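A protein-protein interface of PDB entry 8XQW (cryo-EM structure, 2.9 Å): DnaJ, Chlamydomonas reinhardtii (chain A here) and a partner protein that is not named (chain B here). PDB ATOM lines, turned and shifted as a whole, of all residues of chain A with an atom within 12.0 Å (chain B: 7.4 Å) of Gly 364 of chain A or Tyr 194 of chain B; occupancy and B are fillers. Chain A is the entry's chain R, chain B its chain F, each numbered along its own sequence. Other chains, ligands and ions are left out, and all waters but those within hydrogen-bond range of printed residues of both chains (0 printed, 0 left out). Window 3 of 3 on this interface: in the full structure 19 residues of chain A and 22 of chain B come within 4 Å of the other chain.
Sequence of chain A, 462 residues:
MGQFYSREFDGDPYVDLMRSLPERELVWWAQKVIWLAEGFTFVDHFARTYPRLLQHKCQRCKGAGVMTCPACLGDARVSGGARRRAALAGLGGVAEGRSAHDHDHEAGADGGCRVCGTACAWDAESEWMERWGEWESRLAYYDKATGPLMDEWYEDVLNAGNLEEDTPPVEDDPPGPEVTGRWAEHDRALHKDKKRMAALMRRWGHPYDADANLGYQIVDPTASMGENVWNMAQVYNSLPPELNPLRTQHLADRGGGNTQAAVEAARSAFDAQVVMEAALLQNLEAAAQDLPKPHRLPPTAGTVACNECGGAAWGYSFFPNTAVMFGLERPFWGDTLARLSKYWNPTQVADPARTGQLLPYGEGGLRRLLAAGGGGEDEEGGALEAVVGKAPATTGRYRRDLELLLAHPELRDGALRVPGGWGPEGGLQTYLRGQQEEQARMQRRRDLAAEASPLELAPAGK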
ATOM      1  N   GLN A 357      14.915  -9.577  24.285  1.00  0.00           N
ATOM      2  CA  GLN A 357      14.909 -11.033  24.254  1.00  0.00           C
ATOM      3  C   GLN A 357      13.732 -11.492  23.403  1.00  0.00           C
ATOM      4  O   GLN A 357      12.575 -11.372  23.817  1.00  0.00           O
ATOM      5  CB  GLN A 357      14.824 -11.601  25.665  1.00  0.00           C
ATOM      6  CG  GLN A 357      15.021 -13.090  25.731  1.00  0.00           C
ATOM      7  CD  GLN A 357      14.407 -13.692  26.966  1.00  0.00           C
ATOM      8  OE1 GLN A 357      13.819 -12.991  27.784  1.00  0.00           O
ATOM      9  NE2 GLN A 357      14.537 -15.000  27.106  1.00  0.00           N
ATOM     10  N   LEU A 358      14.026 -12.021  22.219  1.00  0.00           N
ATOM     11  CA  LEU A 358      12.987 -12.394  21.270  1.00  0.00           C
ATOM     12  C   LEU A 358      12.577 -13.853  21.362  1.00  0.00           C
ATOM     13  O   LEU A 358      11.435 -14.186  21.034  1.00  0.00           O
ATOM     14  CB  LEU A 358      13.449 -12.099  19.841  1.00  0.00           C
ATOM     15  CG  LEU A 358      13.796 -10.651  19.498  1.00  0.00           C
ATOM     16  CD1 LEU A 358      13.693 -10.433  17.999  1.00  0.00           C
ATOM     17  CD2 LEU A 358      12.906  -9.670  20.246  1.00  0.00           C
ATOM     18  N   LEU A 359      13.463 -14.718  21.788  1.00  0.00           N
ATOM     19  CA  LEU A 359      13.200 -16.142  21.835  1.00  0.00           C
ATOM     20  C   LEU A 359      13.163 -16.636  23.267  1.00  0.00           C
ATOM     21  O   LEU A 359      13.834 -16.086  24.144  1.00  0.00           O
ATOM     22  CB  LEU A 359      14.281 -16.899  21.065  1.00  0.00           C
ATOM     23  CG  LEU A 359      14.555 -16.381  19.659  1.00  0.00           C
ATOM     24  CD1 LEU A 359      15.786 -17.038  19.086  1.00  0.00           C
ATOM     25  CD2 LEU A 359      13.353 -16.664  18.791  1.00  0.00           C
ATOM     26  N   PRO A 360      12.389 -17.678  23.546  1.00  0.00           N
ATOM     27  CA  PRO A 360      12.475 -18.324  24.855  1.00  0.00           C
ATOM     28  C   PRO A 360      13.861 -18.906  25.077  1.00  0.00           C
ATOM     29  O   PRO A 360      14.670 -19.031  24.158  1.00  0.00           O
ATOM     30  CB  PRO A 360      11.412 -19.423  24.783  1.00  0.00           C
ATOM     31  CG  PRO A 360      11.209 -19.655  23.331  1.00  0.00           C
ATOM     32  CD  PRO A 360      11.395 -18.326  22.679  1.00  0.00           C
ATOM     33  N   TYR A 361      14.131 -19.265  26.327  1.00  0.00           N
ATOM     34  CA  TYR A 361      15.449 -19.768  26.672  1.00  0.00           C
ATOM     35  C   TYR A 361      15.733 -21.069  25.936  1.00  0.00           C
ATOM     36  O   TYR A 361      14.828 -21.734  25.430  1.00  0.00           O
ATOM     37  CB  TYR A 361      15.558 -19.983  28.175  1.00  0.00           C
ATOM     38  CG  TYR A 361      15.378 -18.726  28.985  1.00  0.00           C
ATOM     39  CD1 TYR A 361      16.446 -17.899  29.258  1.00  0.00           C
ATOM     40  CD2 TYR A 361      14.139 -18.373  29.481  1.00  0.00           C
ATOM     41  CE1 TYR A 361      16.283 -16.759  29.996  1.00  0.00           C
ATOM     42  CE2 TYR A 361      13.970 -17.236  30.222  1.00  0.00           C
ATOM     43  CZ  TYR A 361      15.045 -16.435  30.474  1.00  0.00           C
ATOM     44  OH  TYR A 361      14.873 -15.298  31.218  1.00  0.00           O
ATOM     45  N   GLY A 362      17.003 -21.421  25.871  1.00  0.00           N
ATOM     46  CA  GLY A 362      17.458 -22.604  25.183  1.00  0.00           C
ATOM     47  C   GLY A 362      18.557 -22.246  24.218  1.00  0.00           C
ATOM     48  O   GLY A 362      18.938 -21.086  24.081  1.00  0.00           O
ATOM     49  N   GLU A 363      19.077 -23.257  23.533  1.00  0.00           N
ATOM     50  CA  GLU A 363      20.139 -23.071  22.558  1.00  0.00           C
ATOM     51  C   GLU A 363      19.632 -23.410  21.167  1.00  0.00           C
ATOM     52  O   GLU A 363      18.721 -24.225  21.002  1.00  0.00           O
ATOM     53  CB  GLU A 363      21.354 -23.939  22.878  1.00  0.00           C
ATOM     54  CG  GLU A 363      22.125 -23.490  24.094  1.00  0.00           C
ATOM     55  CD  GLU A 363      23.037 -22.322  23.802  1.00  0.00           C
ATOM     56  OE1 GLU A 363      23.737 -21.873  24.729  1.00  0.00           O
ATOM     57  OE2 GLU A 363      23.063 -21.849  22.650  1.00  0.00           O
ATOM     58  N   GLY A 364      20.241 -22.779  20.167  1.00  0.00           N
ATOM     59  CA  GLY A 364      19.879 -23.011  18.784  1.00  0.00           C
ATOM     60  C   GLY A 364      18.406 -22.791  18.521  1.00  0.00           C
ATOM     61  O   GLY A 364      17.726 -23.667  17.977  1.00  0.00           O
ATOM     62  N   GLY A 365      17.899 -21.623  18.913  1.00  0.00           N
ATOM     63  CA  GLY A 365      16.484 -21.350  18.735  1.00  0.00           C
ATOM     64  C   GLY A 365      16.120 -21.032  17.298  1.00  0.00           C
ATOM     65  O   GLY A 365      14.963 -21.167  16.899  1.00  0.00           O
ATOM     66  N   LEU A 366      17.102 -20.611  16.499  1.00  0.00           N
ATOM     67  CA  LEU A 366      16.807 -20.178  15.137  1.00  0.00           C
ATOM     68  C   LEU A 366      16.384 -21.351  14.264  1.00  0.00           C
ATOM     69  O   LEU A 366      15.344 -21.296  13.598  1.00  0.00           O
ATOM     70  CB  LEU A 366      18.015 -19.460  14.543  1.00  0.00           C
ATOM     71  CG  LEU A 366      18.209 -18.024  15.034  1.00  0.00           C
ATOM     72  CD1 LEU A 366      19.271 -17.316  14.217  1.00  0.00           C
ATOM     73  CD2 LEU A 366      16.904 -17.258  14.981  1.00  0.00           C
ATOM     74  N   ARG A 367      17.180 -22.421  14.244  1.00  0.00           N
ATOM     75  CA  ARG A 367      16.762 -23.620  13.525  1.00  0.00           C
ATOM     76  C   ARG A 367      15.476 -24.189  14.104  1.00  0.00           C
ATOM     77  O   ARG A 367      14.668 -24.774  13.374  1.00  0.00           O
ATOM     78  CB  ARG A 367      17.870 -24.671  13.555  1.00  0.00           C
ATOM     79  CG  ARG A 367      19.094 -24.300  12.739  1.00  0.00           C
ATOM     80  CD  ARG A 367      20.169 -23.666  13.606  1.00  0.00           C
ATOM     81  NE  ARG A 367      20.305 -24.343  14.894  1.00  0.00           N
ATOM     82  CZ  ARG A 367      21.041 -25.430  15.097  1.00  0.00           C
ATOM     83  NH1 ARG A 367      21.720 -25.973  14.095  1.00  0.00           N
ATOM     84  NH2 ARG A 367      21.106 -25.973  16.305  1.00  0.00           N
ATOM     85  N   ARG A 368      15.267 -24.018  15.407  1.00  0.00           N
ATOM     86  CA  ARG A 368      14.021 -24.450  16.027  1.00  0.00           C
ATOM     87  C   ARG A 368      12.843 -23.592  15.583  1.00  0.00           C
ATOM     88  O   ARG A 368      11.689 -24.019  15.703  1.00  0.00           O
ATOM     89  CB  ARG A 368      14.161 -24.405  17.548  1.00  0.00           C
ATOM     90  CG  ARG A 368      14.573 -25.718  18.178  1.00  0.00           C
ATOM     91  CD  ARG A 368      13.364 -26.587  18.462  1.00  0.00           C
ATOM     92  NE  ARG A 368      12.399 -25.914  19.328  1.00  0.00           N
ATOM     93  CZ  ARG A 368      11.260 -25.377  18.903  1.00  0.00           C
ATOM     94  NH1 ARG A 368      10.444 -24.781  19.761  1.00  0.00           N
ATOM     95  NH2 ARG A 368      10.940 -25.431  17.618  1.00  0.00           N
ATOM     96  N   LEU A 369      13.106 -22.389  15.081  1.00  0.00           N
ATOM     97  CA  LEU A 369      12.066 -21.434  14.730  1.00  0.00           C
ATOM     98  C   LEU A 369      11.600 -21.559  13.287  1.00  0.00           C
ATOM     99  O   LEU A 369      10.547 -21.012  12.942  1.00  0.00           O
ATOM    100  CB  LEU A 369      12.561 -20.011  14.985  1.00  0.00           C
ATOM    101  CG  LEU A 369      11.496 -18.987  15.369  1.00  0.00           C
ATOM    102  CD1 LEU A 369      10.803 -19.389  16.657  1.00  0.00           C
ATOM    103  CD2 LEU A 369      12.116 -17.613  15.496  1.00  0.00           C
ATOM    104  N   LEU A 370      12.350 -22.257  12.443  1.00  0.00           N
ATOM    105  CA  LEU A 370      11.989 -22.409  11.039  1.00  0.00           C
ATOM    106  C   LEU A 370      10.652 -23.125  10.888  1.00  0.00           C
ATOM    107  O   LEU A 370      10.505 -24.273  11.307  1.00  0.00           O
ATOM    108  CB  LEU A 370      13.077 -23.172  10.285  1.00  0.00           C
ATOM    109  CG  LEU A 370      14.498 -22.624  10.391  1.00  0.00           C
ATOM    110  CD1 LEU A 370      15.387 -23.252   9.333  1.00  0.00           C
ATOM    111  CD2 LEU A 370      14.502 -21.112  10.270  1.00  0.00           C
ATOM    112  N   LEU B 117      31.716 -22.609  25.426  1.00  0.00           N
ATOM    113  CA  LEU B 117      30.343 -22.398  24.990  1.00  0.00           C
ATOM    114  C   LEU B 117      30.290 -21.597  23.696  1.00  0.00           C
ATOM    115  O   LEU B 117      29.558 -21.956  22.766  1.00  0.00           O
ATOM    116  CB  LEU B 117      29.552 -21.694  26.084  1.00  0.00           C
ATOM    117  CG  LEU B 117      28.066 -21.553  25.806  1.00  0.00           C
ATOM    118  CD1 LEU B 117      27.501 -22.870  25.346  1.00  0.00           C
ATOM    119  CD2 LEU B 117      27.379 -21.090  27.056  1.00  0.00           C
ATOM    120  N   ILE B 120      31.432 -23.599  20.736  1.00  0.00           N
ATOM    121  CA  ILE B 120      30.414 -24.521  20.249  1.00  0.00           C
ATOM    122  C   ILE B 120      29.367 -23.772  19.443  1.00  0.00           C
ATOM    123  O   ILE B 120      28.963 -24.213  18.363  1.00  0.00           O
ATOM    124  CB  ILE B 120      29.775 -25.287  21.415  1.00  0.00           C
ATOM    125  CG1 ILE B 120      30.737 -26.343  21.942  1.00  0.00           C
ATOM    126  CG2 ILE B 120      28.501 -25.942  20.960  1.00  0.00           C
ATOM    127  CD1 ILE B 120      30.150 -27.197  23.019  1.00  0.00           C
ATOM    128  N   ARG B 121      28.914 -22.626  19.947  1.00  0.00           N
ATOM    129  CA  ARG B 121      27.863 -21.890  19.256  1.00  0.00           C
ATOM    130  C   ARG B 121      28.314 -21.417  17.882  1.00  0.00           C
ATOM    131  O   ARG B 121      27.559 -21.513  16.911  1.00  0.00           O
ATOM    132  CB  ARG B 121      27.412 -20.704  20.095  1.00  0.00           C
ATOM    133  CG  ARG B 121      26.561 -21.076  21.276  1.00  0.00           C
ATOM    134  CD  ARG B 121      26.367 -19.883  22.168  1.00  0.00           C
ATOM    135  NE  ARG B 121      25.348 -20.110  23.179  1.00  0.00           N
ATOM    136  CZ  ARG B 121      25.175 -19.333  24.238  1.00  0.00           C
ATOM    137  NH1 ARG B 121      25.958 -18.282  24.427  1.00  0.00           N
ATOM    138  NH2 ARG B 121      24.224 -19.610  25.111  1.00  0.00           N
ATOM    139  N   THR B 122      29.534 -20.900  17.776  1.00  0.00           N
ATOM    140  CA  THR B 122      30.023 -20.348  16.520  1.00  0.00           C
ATOM    141  C   THR B 122      30.834 -21.342  15.701  1.00  0.00           C
ATOM    142  O   THR B 122      31.689 -20.921  14.919  1.00  0.00           O
ATOM    143  CB  THR B 122      30.866 -19.103  16.780  1.00  0.00           C
ATOM    144  OG1 THR B 122      31.940 -19.433  17.664  1.00  0.00           O
ATOM    145  CG2 THR B 122      30.022 -18.021  17.413  1.00  0.00           C
ATOM    146  N   GLY B 123      30.610 -22.639  15.876  1.00  0.00           N
ATOM    147  CA  GLY B 123      31.171 -23.642  15.001  1.00  0.00           C
ATOM    148  C   GLY B 123      32.676 -23.774  15.008  1.00  0.00           C
ATOM    149  O   GLY B 123      33.207 -24.578  14.236  1.00  0.00           O
ATOM    150  N   ILE B 125      34.456 -25.236  17.080  1.00  0.00           N
ATOM    151  CA  ILE B 125      34.834 -26.449  17.796  1.00  0.00           C
ATOM    152  C   ILE B 125      34.172 -27.625  17.102  1.00  0.00           C
ATOM    153  O   ILE B 125      32.996 -27.547  16.728  1.00  0.00           O
ATOM    154  CB  ILE B 125      34.426 -26.385  19.273  1.00  0.00           C
ATOM    155  CG1 ILE B 125      35.114 -25.212  19.954  1.00  0.00           C
ATOM    156  CG2 ILE B 125      34.775 -27.669  19.976  1.00  0.00           C
ATOM    157  CD1 ILE B 125      34.893 -25.165  21.431  1.00  0.00           C
ATOM    158  N   ARG B 186      23.797 -25.834  30.034  1.00  0.00           N
ATOM    159  CA  ARG B 186      24.065 -25.072  28.818  1.00  0.00           C
ATOM    160  C   ARG B 186      24.868 -25.889  27.818  1.00  0.00           C
ATOM    161  O   ARG B 186      24.525 -25.948  26.632  1.00  0.00           O
ATOM    162  CB  ARG B 186      24.808 -23.787  29.155  1.00  0.00           C
ATOM    163  CG  ARG B 186      23.920 -22.650  29.554  1.00  0.00           C
ATOM    164  CD  ARG B 186      23.213 -22.050  28.377  1.00  0.00           C
ATOM    165  NE  ARG B 186      22.237 -21.072  28.827  1.00  0.00           N
ATOM    166  CZ  ARG B 186      21.206 -20.668  28.104  1.00  0.00           C
ATOM    167  NH1 ARG B 186      20.355 -19.781  28.590  1.00  0.00           N
ATOM    168  NH2 ARG B 186      21.024 -21.156  26.891  1.00  0.00           N
ATOM    169  N   SER B 188      25.203 -29.090  27.596  1.00  0.00           N
ATOM    170  CA  SER B 188      24.436 -30.222  27.097  1.00  0.00           C
ATOM    171  C   SER B 188      23.465 -29.785  26.012  1.00  0.00           C
ATOM    172  O   SER B 188      23.372 -30.416  24.952  1.00  0.00           O
ATOM    173  CB  SER B 188      23.692 -30.892  28.242  1.00  0.00           C
ATOM    174  OG  SER B 188      24.564 -31.102  29.331  1.00  0.00           O
ATOM    175  N   GLN B 189      22.726 -28.704  26.258  1.00  0.00           N
ATOM    176  CA  GLN B 189      21.813 -28.208  25.238  1.00  0.00           C
ATOM    177  C   GLN B 189      22.562 -27.825  23.972  1.00  0.00           C
ATOM    178  O   GLN B 189      22.096 -28.101  22.863  1.00  0.00           O
ATOM    179  CB  GLN B 189      21.028 -27.016  25.766  1.00  0.00           C
ATOM    180  CG  GLN B 189      19.966 -27.373  26.767  1.00  0.00           C
ATOM    181  CD  GLN B 189      19.109 -26.189  27.122  1.00  0.00           C
ATOM    182  OE1 GLN B 189      19.346 -25.079  26.656  1.00  0.00           O
ATOM    183  NE2 GLN B 189      18.098 -26.416  27.944  1.00  0.00           N
ATOM    184  N   ALA B 190      23.727 -27.196  24.113  1.00  0.00           N
ATOM    185  CA  ALA B 190      24.478 -26.800  22.932  1.00  0.00           C
ATOM    186  C   ALA B 190      24.926 -28.013  22.133  1.00  0.00           C
ATOM    187  O   ALA B 190      24.811 -28.030  20.905  1.00  0.00           O
ATOM    188  CB  ALA B 190      25.677 -25.949  23.331  1.00  0.00           C
ATOM    189  N   LEU B 191      25.430 -29.040  22.811  1.00  0.00           N
ATOM    190  CA  LEU B 191      25.890 -30.225  22.101  1.00  0.00           C
ATOM    191  C   LEU B 191      24.731 -30.962  21.446  1.00  0.00           C
ATOM    192  O   LEU B 191      24.896 -31.570  20.386  1.00  0.00           O
ATOM    193  CB  LEU B 191      26.639 -31.152  23.050  1.00  0.00           C
ATOM    194  CG  LEU B 191      27.970 -30.592  23.528  1.00  0.00           C
ATOM    195  CD1 LEU B 191      28.442 -31.333  24.744  1.00  0.00           C
ATOM    196  CD2 LEU B 191      28.988 -30.687  22.429  1.00  0.00           C
ATOM    197  N   GLN B 192      23.549 -30.922  22.060  1.00  0.00           N
ATOM    198  CA  GLN B 192      22.403 -31.587  21.452  1.00  0.00           C
ATOM    199  C   GLN B 192      21.896 -30.814  20.245  1.00  0.00           C
ATOM    200  O   GLN B 192      21.440 -31.407  19.263  1.00  0.00           O
ATOM    201  CB  GLN B 192      21.288 -31.774  22.475  1.00  0.00           C
ATOM    202  CG  GLN B 192      21.671 -32.667  23.637  1.00  0.00           C
ATOM    203  CD  GLN B 192      20.569 -33.629  24.028  1.00  0.00           C
ATOM    204  OE1 GLN B 192      19.694 -33.946  23.226  1.00  0.00           O
ATOM    205  NE2 GLN B 192      20.600 -34.086  25.274  1.00  0.00           N
ATOM    206  N   GLN B 193      21.966 -29.482  20.296  1.00  0.00           N
ATOM    207  CA  GLN B 193      21.428 -28.688  19.196  1.00  0.00           C
ATOM    208  C   GLN B 193      22.386 -28.617  18.017  1.00  0.00           C
ATOM    209  O   GLN B 193      22.002 -28.952  16.895  1.00  0.00           O
ATOM    210  CB  GLN B 193      21.090 -27.281  19.668  1.00  0.00           C
ATOM    211  CG  GLN B 193      19.977 -27.228  20.681  1.00  0.00           C
ATOM    212  CD  GLN B 193      18.641 -27.590  20.087  1.00  0.00           C
ATOM    213  OE1 GLN B 193      18.453 -27.524  18.876  1.00  0.00           O
ATOM    214  NE2 GLN B 193      17.700 -27.976  20.936  1.00  0.00           N
ATOM    215  N   TYR B 194      23.625 -28.192  18.239  1.00  0.00           N
ATOM    216  CA  TYR B 194      24.550 -27.947  17.144  1.00  0.00           C
ATOM    217  C   TYR B 194      25.256 -29.203  16.659  1.00  0.00           C
ATOM    218  O   TYR B 194      26.089 -29.114  15.754  1.00  0.00           O
ATOM    219  CB  TYR B 194      25.584 -26.902  17.557  1.00  0.00           C
ATOM    220  CG  TYR B 194      24.980 -25.546  17.791  1.00  0.00           C
ATOM    221  CD1 TYR B 194      24.487 -25.196  19.032  1.00  0.00           C
ATOM    222  CD2 TYR B 194      24.900 -24.619  16.773  1.00  0.00           C
ATOM    223  CE1 TYR B 194      23.933 -23.967  19.252  1.00  0.00           C
ATOM    224  CE2 TYR B 194      24.347 -23.382  16.988  1.00  0.00           C
ATOM    225  CZ  TYR B 194      23.866 -23.064  18.230  1.00  0.00           C
ATOM    226  OH  TYR B 194      23.308 -21.831  18.451  1.00  0.00           O
ATOM    227  N   GLY B 195      24.955 -30.361  17.240  1.00  0.00           N
ATOM    228  CA  GLY B 195      25.478 -31.613  16.730  1.00  0.00           C
ATOM    229  C   GLY B 195      26.982 -31.742  16.740  1.00  0.00           C
ATOM    230  O   GLY B 195      27.527 -32.539  15.973  1.00  0.00           O
ATOM    231  N   THR B 196      27.673 -30.969  17.571  1.00  0.00           N
ATOM    232  CA  THR B 196      29.110 -31.132  17.728  1.00  0.00           C
ATOM    233  C   THR B 196      29.427 -32.558  18.159  1.00  0.00           C
ATOM    234  O   THR B 196      28.720 -33.153  18.975  1.00  0.00           O
ATOM    235  CB  THR B 196      29.634 -30.131  18.755  1.00  0.00           C
ATOM    236  OG1 THR B 196      29.750 -28.842  18.146  1.00  0.00           O
ATOM    237  CG2 THR B 196      30.979 -30.549  19.287  1.00  0.00           C
ATOM    238  N   ALA B 197      30.487 -33.126  17.588  1.00  0.00           N
ATOM    239  CA  ALA B 197      30.804 -34.522  17.857  1.00  0.00           C
ATOM    240  C   ALA B 197      31.285 -34.683  19.291  1.00  0.00           C
ATOM    241  O   ALA B 197      32.141 -33.929  19.756  1.00  0.00           O
ATOM    242  CB  ALA B 197      31.861 -35.029  16.882  1.00  0.00           C
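Of the 17 printed residues of chain B, 6 touch a printed residue of chain A.
Among the printed residues, 10 pairs touch across the chains.
OE1 of Glu 363 of chain A lies within salt-bridge range of NE of Arg 121 of chain B.
The guanidinium group (NH2) of Arg 186 of chain B is in salt-bridge range of the side-chain carboxylate (OE1) of Glu 363 of chain A (3.5 Å).
The backbone carbonyl oxygen (O) of Gln 193 of chain B lies within hydrogen-bond range of the guanidinium group (NH2) of Arg 367 of chain A, at 3.2 Å.
Of chain B, only Tyr 194 comes within 4 Å of Gly 364 of chain A.
Tyr 194 of chain B touches two residues of chain A.
No residue of chain A comes within 4 Å of Ile 120 of chain B.
Of chain A, only Glu 363 comes within 4 Å of Arg 121 of chain B.
Of chain A, only Glu 363 (3.3 Å) and Arg 367 (3.2 Å) come within 4 Å of Gln 193 of chain B.
No residue of chain A comes within 4 Å of Gly 195 of chain B.
No residue of chain A comes within 4 Å of Thr 196 of chain B.
Printed residues of chain A within 4 Å of Gln 189 of chain B: Gly 362 and Glu 363.
Of the printed residues of chain B, Gly 362 of chain A touches Arg 186 (3.5 Å) and Gln 189 (3.4 Å).
Printed residues of chain A within 4 Å of Leu 117 of chain B: Glu 363.
Of the printed residues of chain B, Arg 367 of chain A touches Gln 193 (3.2 Å) and Tyr 194 (3.9 Å).
The nearest residue of chain B that does not touch Gly 364 of chain A is Gln 193 of chain B (4.03 Å).
Arg 186 of chain B touches Gly 362 of chain A.
Gln 189 of chain B touches Gly 362 of chain A.
Leu 117 of chain B touches Glu 363 of chain A (CD1 to OE1, 3.9 Å).
Gln 189 of chain B touches Glu 363 of chain A.
Gln 193 of chain B touches Glu 363 of chain A (CG to O, 3.3 Å).
Gly 364 of chain A touches Tyr 194 of chain B.
Arg 367 of chain A touches Tyr 194 of chain B.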
